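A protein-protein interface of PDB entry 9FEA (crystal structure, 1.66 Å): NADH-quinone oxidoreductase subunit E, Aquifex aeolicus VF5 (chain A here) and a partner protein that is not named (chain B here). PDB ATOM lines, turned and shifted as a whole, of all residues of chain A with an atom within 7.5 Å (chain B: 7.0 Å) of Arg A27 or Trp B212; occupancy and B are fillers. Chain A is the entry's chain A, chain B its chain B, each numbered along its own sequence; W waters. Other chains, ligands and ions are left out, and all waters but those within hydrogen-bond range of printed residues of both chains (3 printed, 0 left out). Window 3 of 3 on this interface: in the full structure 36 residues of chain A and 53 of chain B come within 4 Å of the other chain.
NE2 of Gln A28 lies within hydrogen-bond range of OH of Tyr B131, 3.2 Å away. O of Gly B194 lies close to NE2 of His A62, at 3.3 Å. The side-chain amide nitrogen of Gln A28 sits at hydrogen-bond distance from the backbone carbonyl oxygen of Leu B192, 3.1 Å away.
The side-chain carboxylate (OE1) of Glu B193 is in salt-bridge range of the side-chain amino group (NZ) of Lys B195 (2.8 Å). OE2 of Glu B193 is in salt-bridge range of NH2 of Arg B200. The backbone NH (N) of Trp B212 lies within hydrogen-bond range of the side-chain carboxylate (OE2) of Glu B193 (2.8 Å). The side-chain amide oxygen (OE1) of Gln A28 is in hydrogen-bond range of the backbone NH (N) of Lys A25.
Among the printed residues, pairs that only touch across the chains: Pro A24 with Glu B129, Arg A27 with Gly B194, Leu A31 with Ser B191, Arg A27 with Trp B212, Lys A25 with Trp B212, Ile A30 with Gly B194, Arg A27 with Glu B193, Gln A28 with Trp B212, Pro A24 with Tyr B131, Phe A23 with Tyr B131 and His A62 with Lys B195.
Arg A27 touches just these residues of chain B: Glu B193 (3.7 Å), Gly B194 (3.4 Å) and Trp B212 (3.5 Å). Printed residues of chain B within 4 Å of Leu A31: Ser B191. Printed residues of chain A within 4 Å of Glu B193: Arg A27. Of the printed residues of chain A, Lys B195 touches His A62. The nearest residue of chain B that does not touch Arg A27 is Leu B192 (5.6 Å). The nearest printed residue of chain A that does not touch Glu B193 is Gln A28 (4.8 Å).
Printed residues of chain B that touch a printed residue of chain A: Glu B129, Tyr B131, Ser B191, Leu B192, Glu B193, Gly B194, Lys B195 and Trp B212. Along chain B the printed residues that touch a printed residue of chain A span positions 129 to 212. Of the 15 printed residues of chain A, 8 touch a printed residue of chain B. Among the printed residues, 14 pairs touch across the chains.
Water W1 lies within hydrogen-bond range of O of Glu B193 (2.7 Å) and NE of Arg A27 (2.8 Å). Water W3 lies within hydrogen-bond range of the backbone carbonyl oxygen of Ser B191 (2.8 Å) and the backbone carbonyl oxygen of Gln A28 (3.4 Å). Water W2 lies within hydrogen-bond range of the indole nitrogen of Trp B212 (2.8 Å), the side-chain carboxylate of Glu B129 (2.8 Å), the side-chain amide oxygen of Gln A28 (2.8 Å) and the side-chain hydroxyl of Tyr B131 (3.0 Å).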
ATOM      1  N   ILE A  20      16.531 -32.531  -5.685  1.00  0.00           N
ATOM      2  CA  ILE A  20      15.766 -32.071  -4.533  1.00  0.00           C
ATOM      3  C   ILE A  20      16.699 -31.544  -3.435  1.00  0.00           C
ATOM      4  O   ILE A  20      16.342 -30.600  -2.732  1.00  0.00           O
ATOM      5  CB  ILE A  20      14.802 -33.183  -4.066  1.00  0.00           C
ATOM      6  CG1 ILE A  20      13.620 -33.280  -5.034  1.00  0.00           C
ATOM      7  CG2 ILE A  20      14.333 -32.987  -2.623  1.00  0.00           C
ATOM      8  CD1 ILE A  20      12.824 -34.559  -4.931  1.00  0.00           C
ATOM      9  N   PHE A  23      18.973 -27.348  -4.252  1.00  0.00           N
ATOM     10  CA  PHE A  23      18.595 -26.009  -3.830  1.00  0.00           C
ATOM     11  C   PHE A  23      18.359 -25.974  -2.320  1.00  0.00           C
ATOM     12  O   PHE A  23      18.199 -27.018  -1.683  1.00  0.00           O
ATOM     13  CB  PHE A  23      17.326 -25.532  -4.533  1.00  0.00           C
ATOM     14  CG  PHE A  23      17.436 -25.425  -6.042  1.00  0.00           C
ATOM     15  CD1 PHE A  23      18.060 -24.333  -6.627  1.00  0.00           C
ATOM     16  CD2 PHE A  23      16.853 -26.371  -6.867  1.00  0.00           C
ATOM     17  CE1 PHE A  23      18.140 -24.220  -8.004  1.00  0.00           C
ATOM     18  CE2 PHE A  23      16.944 -26.254  -8.246  1.00  0.00           C
ATOM     19  CZ  PHE A  23      17.573 -25.174  -8.806  1.00  0.00           C
ATOM     20  N   PRO A  24      18.354 -24.776  -1.685  1.00  0.00           N
ATOM     21  CA  PRO A  24      18.063 -24.688  -0.255  1.00  0.00           C
ATOM     22  C   PRO A  24      16.714 -25.284   0.141  1.00  0.00           C
ATOM     23  O   PRO A  24      16.611 -25.841   1.218  1.00  0.00           O
ATOM     24  CB  PRO A  24      18.160 -23.188   0.023  1.00  0.00           C
ATOM     25  CG  PRO A  24      19.174 -22.717  -0.993  1.00  0.00           C
ATOM     26  CD  PRO A  24      18.811 -23.494  -2.245  1.00  0.00           C
ATOM     27  N   LYS A  25      15.692 -25.158  -0.729  1.00  0.00           N
ATOM     28  CA  LYS A  25      14.364 -25.660  -0.411  1.00  0.00           C
ATOM     29  C   LYS A  25      13.975 -26.699  -1.459  1.00  0.00           C
ATOM     30  O   LYS A  25      14.257 -26.527  -2.633  1.00  0.00           O
ATOM     31  CB  LYS A  25      13.349 -24.508  -0.341  1.00  0.00           C
ATOM     32  CG  LYS A  25      13.666 -23.380   0.629  1.00  0.00           C
ATOM     33  CD  LYS A  25      12.469 -22.488   0.920  1.00  0.00           C
ATOM     34  CE  LYS A  25      12.873 -21.292   1.718  1.00  0.00           C
ATOM     35  NZ  LYS A  25      11.724 -20.488   2.149  1.00  0.00           N
ATOM     36  N   LYS A  26      13.312 -27.775  -1.033  1.00  0.00           N
ATOM     37  CA  LYS A  26      13.032 -28.899  -1.908  1.00  0.00           C
ATOM     38  C   LYS A  26      12.173 -28.484  -3.103  1.00  0.00           C
ATOM     39  O   LYS A  26      12.409 -28.936  -4.224  1.00  0.00           O
ATOM     40  CB  LYS A  26      12.269 -29.996  -1.159  1.00  0.00           C
ATOM     41  CG  LYS A  26      13.015 -30.643   0.005  1.00  0.00           C
ATOM     42  CD  LYS A  26      12.227 -31.804   0.603  1.00  0.00           C
ATOM     43  CE  LYS A  26      12.715 -32.265   1.947  1.00  0.00           C
ATOM     44  NZ  LYS A  26      14.084 -32.784   1.872  1.00  0.00           N
ATOM     45  N   ARG A  27      11.173 -27.632  -2.860  1.00  0.00           N
ATOM     46  CA  ARG A  27      10.204 -27.299  -3.896  1.00  0.00           C
ATOM     47  C   ARG A  27      10.843 -26.560  -5.071  1.00  0.00           C
ATOM     48  O   ARG A  27      10.261 -26.529  -6.147  1.00  0.00           O
ATOM     49  CB  ARG A  27       9.022 -26.513  -3.327  1.00  0.00           C
ATOM     50  CG  ARG A  27       9.318 -25.135  -2.758  1.00  0.00           C
ATOM     51  CD  ARG A  27       8.162 -24.794  -1.835  1.00  0.00           C
ATOM     52  NE  ARG A  27       8.269 -23.543  -1.079  1.00  0.00           N
ATOM     53  CZ  ARG A  27       8.708 -23.425   0.166  1.00  0.00           C
ATOM     54  NH1 ARG A  27       8.590 -22.275   0.802  1.00  0.00           N
ATOM     55  NH2 ARG A  27       9.261 -24.449   0.786  1.00  0.00           N
ATOM     56  N   GLN A  28      12.039 -25.989  -4.881  1.00  0.00           N
ATOM     57  CA  GLN A  28      12.729 -25.290  -5.949  1.00  0.00           C
ATOM     58  C   GLN A  28      13.146 -26.245  -7.060  1.00  0.00           C
ATOM     59  O   GLN A  28      13.371 -25.790  -8.183  1.00  0.00           O
ATOM     60  CB  GLN A  28      13.944 -24.529  -5.423  1.00  0.00           C
ATOM     61  CG  GLN A  28      13.568 -23.550  -4.320  1.00  0.00           C
ATOM     62  CD  GLN A  28      14.727 -22.678  -3.927  1.00  0.00           C
ATOM     63  OE1 GLN A  28      15.430 -22.959  -2.949  1.00  0.00           O
ATOM     64  NE2 GLN A  28      14.968 -21.662  -4.734  1.00  0.00           N
ATOM     65  N   ALA A  29      13.239 -27.541  -6.742  1.00  0.00           N
ATOM     66  CA  ALA A  29      13.742 -28.544  -7.667  1.00  0.00           C
ATOM     67  C   ALA A  29      12.676 -29.038  -8.646  1.00  0.00           C
ATOM     68  O   ALA A  29      12.980 -29.880  -9.484  1.00  0.00           O
ATOM     69  CB  ALA A  29      14.330 -29.701  -6.891  1.00  0.00           C
ATOM     70  N   ILE A  30      11.459 -28.490  -8.587  1.00  0.00           N
ATOM     71  CA  ILE A  30      10.333 -29.081  -9.309  1.00  0.00           C
ATOM     72  C   ILE A  30      10.610 -29.173 -10.818  1.00  0.00           C
ATOM     73  O   ILE A  30      10.330 -30.203 -11.432  1.00  0.00           O
ATOM     74  CB  ILE A  30       9.019 -28.335  -9.021  1.00  0.00           C
ATOM     75  CG1 ILE A  30       7.823 -29.037  -9.684  1.00  0.00           C
ATOM     76  CG2 ILE A  30       9.112 -26.865  -9.417  1.00  0.00           C
ATOM     77  CD1 ILE A  30       6.469 -28.560  -9.186  1.00  0.00           C
ATOM     78  N   LEU A  31      11.131 -28.111 -11.441  1.00  0.00           N
ATOM     79  CA  LEU A  31      11.323 -28.153 -12.888  1.00  0.00           C
ATOM     80  C   LEU A  31      12.481 -29.077 -13.276  1.00  0.00           C
ATOM     81  O   LEU A  31      12.421 -29.755 -14.295  1.00  0.00           O
ATOM     82  CB  LEU A  31      11.540 -26.746 -13.425  1.00  0.00           C
ATOM     83  CG  LEU A  31      10.415 -25.733 -13.200  1.00  0.00           C
ATOM     84  CD1 LEU A  31      10.724 -24.433 -13.896  1.00  0.00           C
ATOM     85  CD2 LEU A  31       9.066 -26.227 -13.666  1.00  0.00           C
ATOM     86  N   MET A  55       7.904 -36.293  -2.918  1.00  0.00           N
ATOM     87  CA  MET A  55       9.332 -36.026  -2.750  1.00  0.00           C
ATOM     88  C   MET A  55       9.582 -34.529  -2.567  1.00  0.00           C
ATOM     89  O   MET A  55      10.494 -34.134  -1.847  1.00  0.00           O
ATOM     90  CB  MET A  55      10.156 -36.549  -3.939  1.00  0.00           C
ATOM     91  CG  MET A  55      10.139 -38.075  -4.086  1.00  0.00           C
ATOM     92  SD  MET A  55      11.142 -38.736  -5.434  1.00  0.00           S
ATOM     93  CE  MET A  55      10.354 -37.836  -6.767  1.00  0.00           C
ATOM     94  N   LEU A  56       8.753 -33.706  -3.209  1.00  0.00           N
ATOM     95  CA  LEU A  56       8.880 -32.259  -3.144  1.00  0.00           C
ATOM     96  C   LEU A  56       8.165 -31.685  -1.922  1.00  0.00           C
ATOM     97  O   LEU A  56       8.312 -30.496  -1.641  1.00  0.00           O
ATOM     98  CB  LEU A  56       8.292 -31.685  -4.430  1.00  0.00           C
ATOM     99  CG  LEU A  56       9.076 -31.973  -5.716  1.00  0.00           C
ATOM    100  CD1 LEU A  56       8.264 -31.579  -6.925  1.00  0.00           C
ATOM    101  CD2 LEU A  56      10.402 -31.246  -5.727  1.00  0.00           C
ATOM    102  N   GLU A  57       7.364 -32.519  -1.249  1.00  0.00           N
ATOM    103  CA  GLU A  57       6.480 -32.099  -0.168  1.00  0.00           C
ATOM    104  C   GLU A  57       5.541 -31.005  -0.670  1.00  0.00           C
ATOM    105  O   GLU A  57       5.336 -30.000   0.004  1.00  0.00           O
ATOM    106  CB  GLU A  57       7.278 -31.671   1.067  1.00  0.00           C
ATOM    107  CG  GLU A  57       8.045 -32.827   1.707  1.00  0.00           C
ATOM    108  CD  GLU A  57       9.062 -32.447   2.772  1.00  0.00           C
ATOM    109  OE1 GLU A  57       9.184 -31.253   3.132  1.00  0.00           O
ATOM    110  OE2 GLU A  57       9.772 -33.373   3.216  1.00  0.00           O
ATOM    111  N   LEU A  58       4.962 -31.232  -1.858  1.00  0.00           N
ATOM    112  CA  LEU A  58       3.969 -30.341  -2.440  1.00  0.00           C
ATOM    113  C   LEU A  58       2.649 -31.073  -2.649  1.00  0.00           C
ATOM    114  O   LEU A  58       2.627 -32.280  -2.867  1.00  0.00           O
ATOM    115  CB  LEU A  58       4.459 -29.817  -3.785  1.00  0.00           C
ATOM    116  CG  LEU A  58       5.626 -28.838  -3.739  1.00  0.00           C
ATOM    117  CD1 LEU A  58       5.918 -28.416  -5.159  1.00  0.00           C
ATOM    118  CD2 LEU A  58       5.338 -27.644  -2.844  1.00  0.00           C
ATOM    119  N   HIS A  62      -0.641 -28.808  -7.071  1.00  0.00           N
ATOM    120  CA  HIS A  62       0.414 -27.858  -7.383  1.00  0.00           C
ATOM    121  C   HIS A  62       1.280 -28.395  -8.517  1.00  0.00           C
ATOM    122  O   HIS A  62       1.603 -27.660  -9.460  1.00  0.00           O
ATOM    123  CB  HIS A  62       1.147 -27.524  -6.083  1.00  0.00           C
ATOM    124  CG  HIS A  62       2.297 -26.598  -6.211  1.00  0.00           C
ATOM    125  ND1 HIS A  62       3.166 -26.619  -7.281  1.00  0.00           N
ATOM    126  CD2 HIS A  62       2.763 -25.679  -5.376  1.00  0.00           C
ATOM    127  CE1 HIS A  62       4.097 -25.709  -7.095  1.00  0.00           C
ATOM    128  NE2 HIS A  62       3.888 -25.130  -5.959  1.00  0.00           N
ATOM    129  N   TYR B  88      19.263 -11.688  -2.007  1.00  0.00           N
ATOM    130  CA  TYR B  88      19.524 -12.660  -3.039  1.00  0.00           C
ATOM    131  C   TYR B  88      19.919 -11.938  -4.319  1.00  0.00           C
ATOM    132  O   TYR B  88      19.412 -10.861  -4.617  1.00  0.00           O
ATOM    133  CB  TYR B  88      18.305 -13.540  -3.300  1.00  0.00           C
ATOM    134  CG  TYR B  88      17.875 -14.309  -2.069  1.00  0.00           C
ATOM    135  CD1 TYR B  88      18.687 -15.311  -1.556  1.00  0.00           C
ATOM    136  CD2 TYR B  88      16.671 -14.046  -1.428  1.00  0.00           C
ATOM    137  CE1 TYR B  88      18.328 -16.009  -0.419  1.00  0.00           C
ATOM    138  CE2 TYR B  88      16.287 -14.759  -0.303  1.00  0.00           C
ATOM    139  CZ  TYR B  88      17.123 -15.739   0.202  1.00  0.00           C
ATOM    140  OH  TYR B  88      16.769 -16.418   1.333  1.00  0.00           O
ATOM    141  N   GLU B 129      23.692 -16.136  -1.485  1.00  0.00           N
ATOM    142  CA  GLU B 129      23.001 -17.115  -2.307  1.00  0.00           C
ATOM    143  C   GLU B 129      22.629 -16.429  -3.615  1.00  0.00           C
ATOM    144  O   GLU B 129      21.877 -15.458  -3.577  1.00  0.00           O
ATOM    145  CB  GLU B 129      21.793 -17.615  -1.515  1.00  0.00           C
ATOM    146  CG  GLU B 129      20.774 -18.436  -2.305  1.00  0.00           C
ATOM    147  CD  GLU B 129      19.657 -19.024  -1.448  1.00  0.00           C
ATOM    148  OE1 GLU B 129      19.783 -18.999  -0.203  1.00  0.00           O
ATOM    149  OE2 GLU B 129      18.638 -19.489  -1.998  1.00  0.00           O
ATOM    150  N   TYR B 131      21.563 -17.039  -7.974  1.00  0.00           N
ATOM    151  CA  TYR B 131      20.928 -17.953  -8.902  1.00  0.00           C
ATOM    152  C   TYR B 131      21.186 -17.506 -10.329  1.00  0.00           C
ATOM    153  O   TYR B 131      21.292 -16.310 -10.593  1.00  0.00           O
ATOM    154  CB  TYR B 131      19.411 -17.939  -8.740  1.00  0.00           C
ATOM    155  CG  TYR B 131      18.983 -18.536  -7.424  1.00  0.00           C
ATOM    156  CD1 TYR B 131      19.004 -17.808  -6.242  1.00  0.00           C
ATOM    157  CD2 TYR B 131      18.594 -19.860  -7.383  1.00  0.00           C
ATOM    158  CE1 TYR B 131      18.577 -18.377  -5.057  1.00  0.00           C
ATOM    159  CE2 TYR B 131      18.206 -20.450  -6.208  1.00  0.00           C
ATOM    160  CZ  TYR B 131      18.200 -19.709  -5.045  1.00  0.00           C
ATOM    161  OH  TYR B 131      17.788 -20.348  -3.928  1.00  0.00           O
ATOM    162  N   ILE B 189      11.100 -15.189 -10.349  1.00  0.00           N
ATOM    163  CA  ILE B 189      11.206 -15.469  -8.926  1.00  0.00           C
ATOM    164  C   ILE B 189      10.130 -16.491  -8.539  1.00  0.00           C
ATOM    165  O   ILE B 189      10.410 -17.439  -7.823  1.00  0.00           O
ATOM    166  CB  ILE B 189      11.113 -14.173  -8.102  1.00  0.00           C
ATOM    167  CG1 ILE B 189      12.354 -13.306  -8.312  1.00  0.00           C
ATOM    168  CG2 ILE B 189      10.842 -14.475  -6.625  1.00  0.00           C
ATOM    169  CD1 ILE B 189      12.201 -11.861  -7.867  1.00  0.00           C
ATOM    170  N   SER B 191       8.945 -18.796 -10.378  1.00  0.00           N
ATOM    171  CA  SER B 191       9.428 -20.065 -10.911  1.00  0.00           C
ATOM    172  C   SER B 191      10.552 -20.622 -10.031  1.00  0.00           C
ATOM    173  O   SER B 191      10.610 -21.821  -9.747  1.00  0.00           O
ATOM    174  CB  SER B 191       9.863 -19.909 -12.337  1.00  0.00           C
ATOM    175  OG  SER B 191      10.172 -21.147 -12.969  1.00  0.00           O
ATOM    176  N   LEU B 192      11.422 -19.738  -9.546  1.00  0.00           N
ATOM    177  CA  LEU B 192      12.482 -20.154  -8.642  1.00  0.00           C
ATOM    178  C   LEU B 192      11.902 -20.700  -7.343  1.00  0.00           C
ATOM    179  O   LEU B 192      12.559 -21.506  -6.709  1.00  0.00           O
ATOM    180  CB  LEU B 192      13.428 -19.001  -8.316  1.00  0.00           C
ATOM    181  CG  LEU B 192      14.586 -18.779  -9.272  1.00  0.00           C
ATOM    182  CD1 LEU B 192      15.286 -17.501  -8.833  1.00  0.00           C
ATOM    183  CD2 LEU B 192      15.533 -19.992  -9.310  1.00  0.00           C
ATOM    184  N   GLU B 193      10.710 -20.227  -6.930  1.00  0.00           N
ATOM    185  CA  GLU B 193      10.045 -20.660  -5.718  1.00  0.00           C
ATOM    186  C   GLU B 193       9.234 -21.934  -5.966  1.00  0.00           C
ATOM    187  O   GLU B 193       8.520 -22.401  -5.073  1.00  0.00           O
ATOM    188  CB  GLU B 193       9.160 -19.545  -5.161  1.00  0.00           C
ATOM    189  CG  GLU B 193       9.916 -18.309  -4.674  1.00  0.00           C
ATOM    190  CD  GLU B 193       9.031 -17.193  -4.121  1.00  0.00           C
ATOM    191  OE1 GLU B 193       7.797 -17.368  -4.178  1.00  0.00           O
ATOM    192  OE2 GLU B 193       9.545 -16.170  -3.593  1.00  0.00           O
ATOM    193  N   GLY B 194       9.350 -22.488  -7.173  1.00  0.00           N
ATOM    194  CA  GLY B 194       8.740 -23.768  -7.508  1.00  0.00           C
ATOM    195  C   GLY B 194       7.282 -23.649  -7.941  1.00  0.00           C
ATOM    196  O   GLY B 194       6.544 -24.625  -7.877  1.00  0.00           O
ATOM    197  N   LYS B 195       6.895 -22.475  -8.444  1.00  0.00           N
ATOM    198  CA  LYS B 195       5.528 -22.226  -8.885  1.00  0.00           C
ATOM    199  C   LYS B 195       5.430 -21.890 -10.374  1.00  0.00           C
ATOM    200  O   LYS B 195       6.424 -21.799 -11.096  1.00  0.00           O
ATOM    201  CB  LYS B 195       4.988 -21.032  -8.095  1.00  0.00           C
ATOM    202  CG  LYS B 195       4.745 -21.357  -6.635  1.00  0.00           C
ATOM    203  CD  LYS B 195       4.347 -20.155  -5.795  1.00  0.00           C
ATOM    204  CE  LYS B 195       5.522 -19.333  -5.439  1.00  0.00           C
ATOM    205  NZ  LYS B 195       5.146 -18.192  -4.605  1.00  0.00           N
ATOM    206  N   ARG B 200       3.994 -10.802 -10.550  1.00  0.00           N
ATOM    207  CA  ARG B 200       3.394 -10.169  -9.386  1.00  0.00           C
ATOM    208  C   ARG B 200       3.176  -8.692  -9.684  1.00  0.00           C
ATOM    209  O   ARG B 200       3.951  -8.077 -10.406  1.00  0.00           O
ATOM    210  CB  ARG B 200       4.351 -10.228  -8.188  1.00  0.00           C
ATOM    211  CG  ARG B 200       4.907 -11.587  -7.797  1.00  0.00           C
ATOM    212  CD  ARG B 200       5.943 -11.457  -6.675  1.00  0.00           C
ATOM    213  NE  ARG B 200       6.459 -12.752  -6.207  1.00  0.00           N
ATOM    214  CZ  ARG B 200       7.464 -12.899  -5.330  1.00  0.00           C
ATOM    215  NH1 ARG B 200       8.142 -11.853  -4.870  1.00  0.00           N
ATOM    216  NH2 ARG B 200       7.785 -14.113  -4.915  1.00  0.00           N
ATOM    217  N   LYS B 209      10.961  -6.643  -2.084  1.00  0.00           N
ATOM    218  CA  LYS B 209      10.338  -7.920  -1.787  1.00  0.00           C
ATOM    219  C   LYS B 209      10.466  -8.808  -3.017  1.00  0.00           C
ATOM    220  O   LYS B 209       9.831  -8.556  -4.046  1.00  0.00           O
ATOM    221  CB  LYS B 209       8.852  -7.821  -1.432  1.00  0.00           C
ATOM    222  CG  LYS B 209       8.560  -7.151  -0.116  1.00  0.00           C
ATOM    223  CD  LYS B 209       7.090  -7.231   0.299  1.00  0.00           C
ATOM    224  CE  LYS B 209       6.741  -6.154   1.287  1.00  0.00           C
ATOM    225  NZ  LYS B 209       7.632  -6.141   2.453  1.00  0.00           N
ATOM    226  N   GLY B 210      11.319  -9.829  -2.897  1.00  0.00           N
ATOM    227  CA  GLY B 210      11.675 -10.668  -4.017  1.00  0.00           C
ATOM    228  C   GLY B 210      11.551 -12.147  -3.665  1.00  0.00           C
ATOM    229  O   GLY B 210      10.495 -12.611  -3.248  1.00  0.00           O
ATOM    230  N   LEU B 211      12.658 -12.879  -3.808  1.00  0.00           N
ATOM    231  CA  LEU B 211      12.660 -14.296  -3.493  1.00  0.00           C
ATOM    232  C   LEU B 211      12.429 -14.493  -2.000  1.00  0.00           C
ATOM    233  O   LEU B 211      13.136 -13.909  -1.190  1.00  0.00           O
ATOM    234  CB  LEU B 211      13.990 -14.890  -3.946  1.00  0.00           C
ATOM    235  CG  LEU B 211      14.206 -16.381  -3.685  1.00  0.00           C
ATOM    236  CD1 LEU B 211      13.245 -17.189  -4.530  1.00  0.00           C
ATOM    237  CD2 LEU B 211      15.609 -16.785  -4.034  1.00  0.00           C
ATOM    238  N   TRP B 212      11.418 -15.297  -1.660  1.00  0.00           N
ATOM    239  CA  TRP B 212      11.010 -15.540  -0.287  1.00  0.00           C
ATOM    240  C   TRP B 212      10.697 -14.219   0.414  1.00  0.00           C
ATOM    241  O   TRP B 212      10.741 -14.140   1.637  1.00  0.00           O
ATOM    242  CB  TRP B 212      12.067 -16.357   0.475  1.00  0.00           C
ATOM    243  CG  TRP B 212      12.559 -17.568  -0.274  1.00  0.00           C
ATOM    244  CD1 TRP B 212      13.856 -17.883  -0.538  1.00  0.00           C
ATOM    245  CD2 TRP B 212      11.762 -18.635  -0.833  1.00  0.00           C
ATOM    246  NE1 TRP B 212      13.924 -19.045  -1.255  1.00  0.00           N
ATOM    247  CE2 TRP B 212      12.660 -19.544  -1.427  1.00  0.00           C
ATOM    248  CE3 TRP B 212      10.388 -18.919  -0.864  1.00  0.00           C
ATOM    249  CZ2 TRP B 212      12.231 -20.692  -2.079  1.00  0.00           C
ATOM    250  CZ3 TRP B 212       9.965 -20.071  -1.489  1.00  0.00           C
ATOM    251  CH2 TRP B 212      10.878 -20.933  -2.107  1.00  0.00           C
ATOM    252  N   GLY B 213      10.319 -13.206  -0.382  1.00  0.00           N
ATOM    253  CA  GLY B 213       9.907 -11.902   0.105  1.00  0.00           C
ATOM    254  C   GLY B 213      11.081 -11.053   0.596  1.00  0.00           C
ATOM    255  O   GLY B 213      10.868 -10.037   1.255  1.00  0.00           O
ATOM    256  N   LYS B 214      12.302 -11.479   0.284  1.00  0.00           N
ATOM    257  CA  LYS B 214      13.503 -10.781   0.723  1.00  0.00           C
ATOM    258  C   LYS B 214      14.030  -9.903  -0.405  1.00  0.00           C
ATOM    259  O   LYS B 214      13.791 -10.177  -1.589  1.00  0.00           O
ATOM    260  CB  LYS B 214      14.564 -11.811   1.128  1.00  0.00           C
ATOM    261  CG  LYS B 214      14.183 -12.766   2.264  1.00  0.00           C
ATOM    262  CD  LYS B 214      13.658 -12.063   3.509  1.00  0.00           C
ATOM    263  CE  LYS B 214      13.503 -13.000   4.674  1.00  0.00           C
ATOM    264  NZ  LYS B 214      12.756 -12.393   5.781  1.00  0.00           N
ATOM    265  N   PRO B 215      14.855  -8.877  -0.082  1.00  0.00           N
ATOM    266  CA  PRO B 215      15.480  -8.035  -1.092  1.00  0.00           C
ATOM    267  C   PRO B 215      16.237  -8.896  -2.077  1.00  0.00           C
ATOM    268  O   PRO B 215      17.096  -9.679  -1.683  1.00  0.00           O
ATOM    269  CB  PRO B 215      16.418  -7.138  -0.298  1.00  0.00           C
ATOM    270  CG  PRO B 215      15.740  -7.046   1.035  1.00  0.00           C
ATOM    271  CD  PRO B 215      15.236  -8.462   1.275  1.00  0.00           C
ATOM    272  N   THR B 216      15.942  -8.663  -3.353  1.00  0.00           N
ATOM    273  CA  THR B 216      16.460  -9.465  -4.437  1.00  0.00           C
ATOM    274  C   THR B 216      16.813  -8.547  -5.606  1.00  0.00           C
ATOM    275  O   THR B 216      15.988  -7.741  -6.044  1.00  0.00           O
ATOM    276  CB  THR B 216      15.410 -10.493  -4.858  1.00  0.00           C
ATOM    277  OG1 THR B 216      15.068 -11.336  -3.759  1.00  0.00           O
ATOM    278  CG2 THR B 216      15.868 -11.347  -6.023  1.00  0.00           C
HETATM  279  O   HOH W   1       6.993 -21.906  -2.951  1.00  0.00           O
HETATM  280  O   HOH W   2      16.163 -20.681  -1.402  1.00  0.00           O
HETATM  281  O   HOH W   3      12.970 -23.157 -10.244  1.00  0.00           O
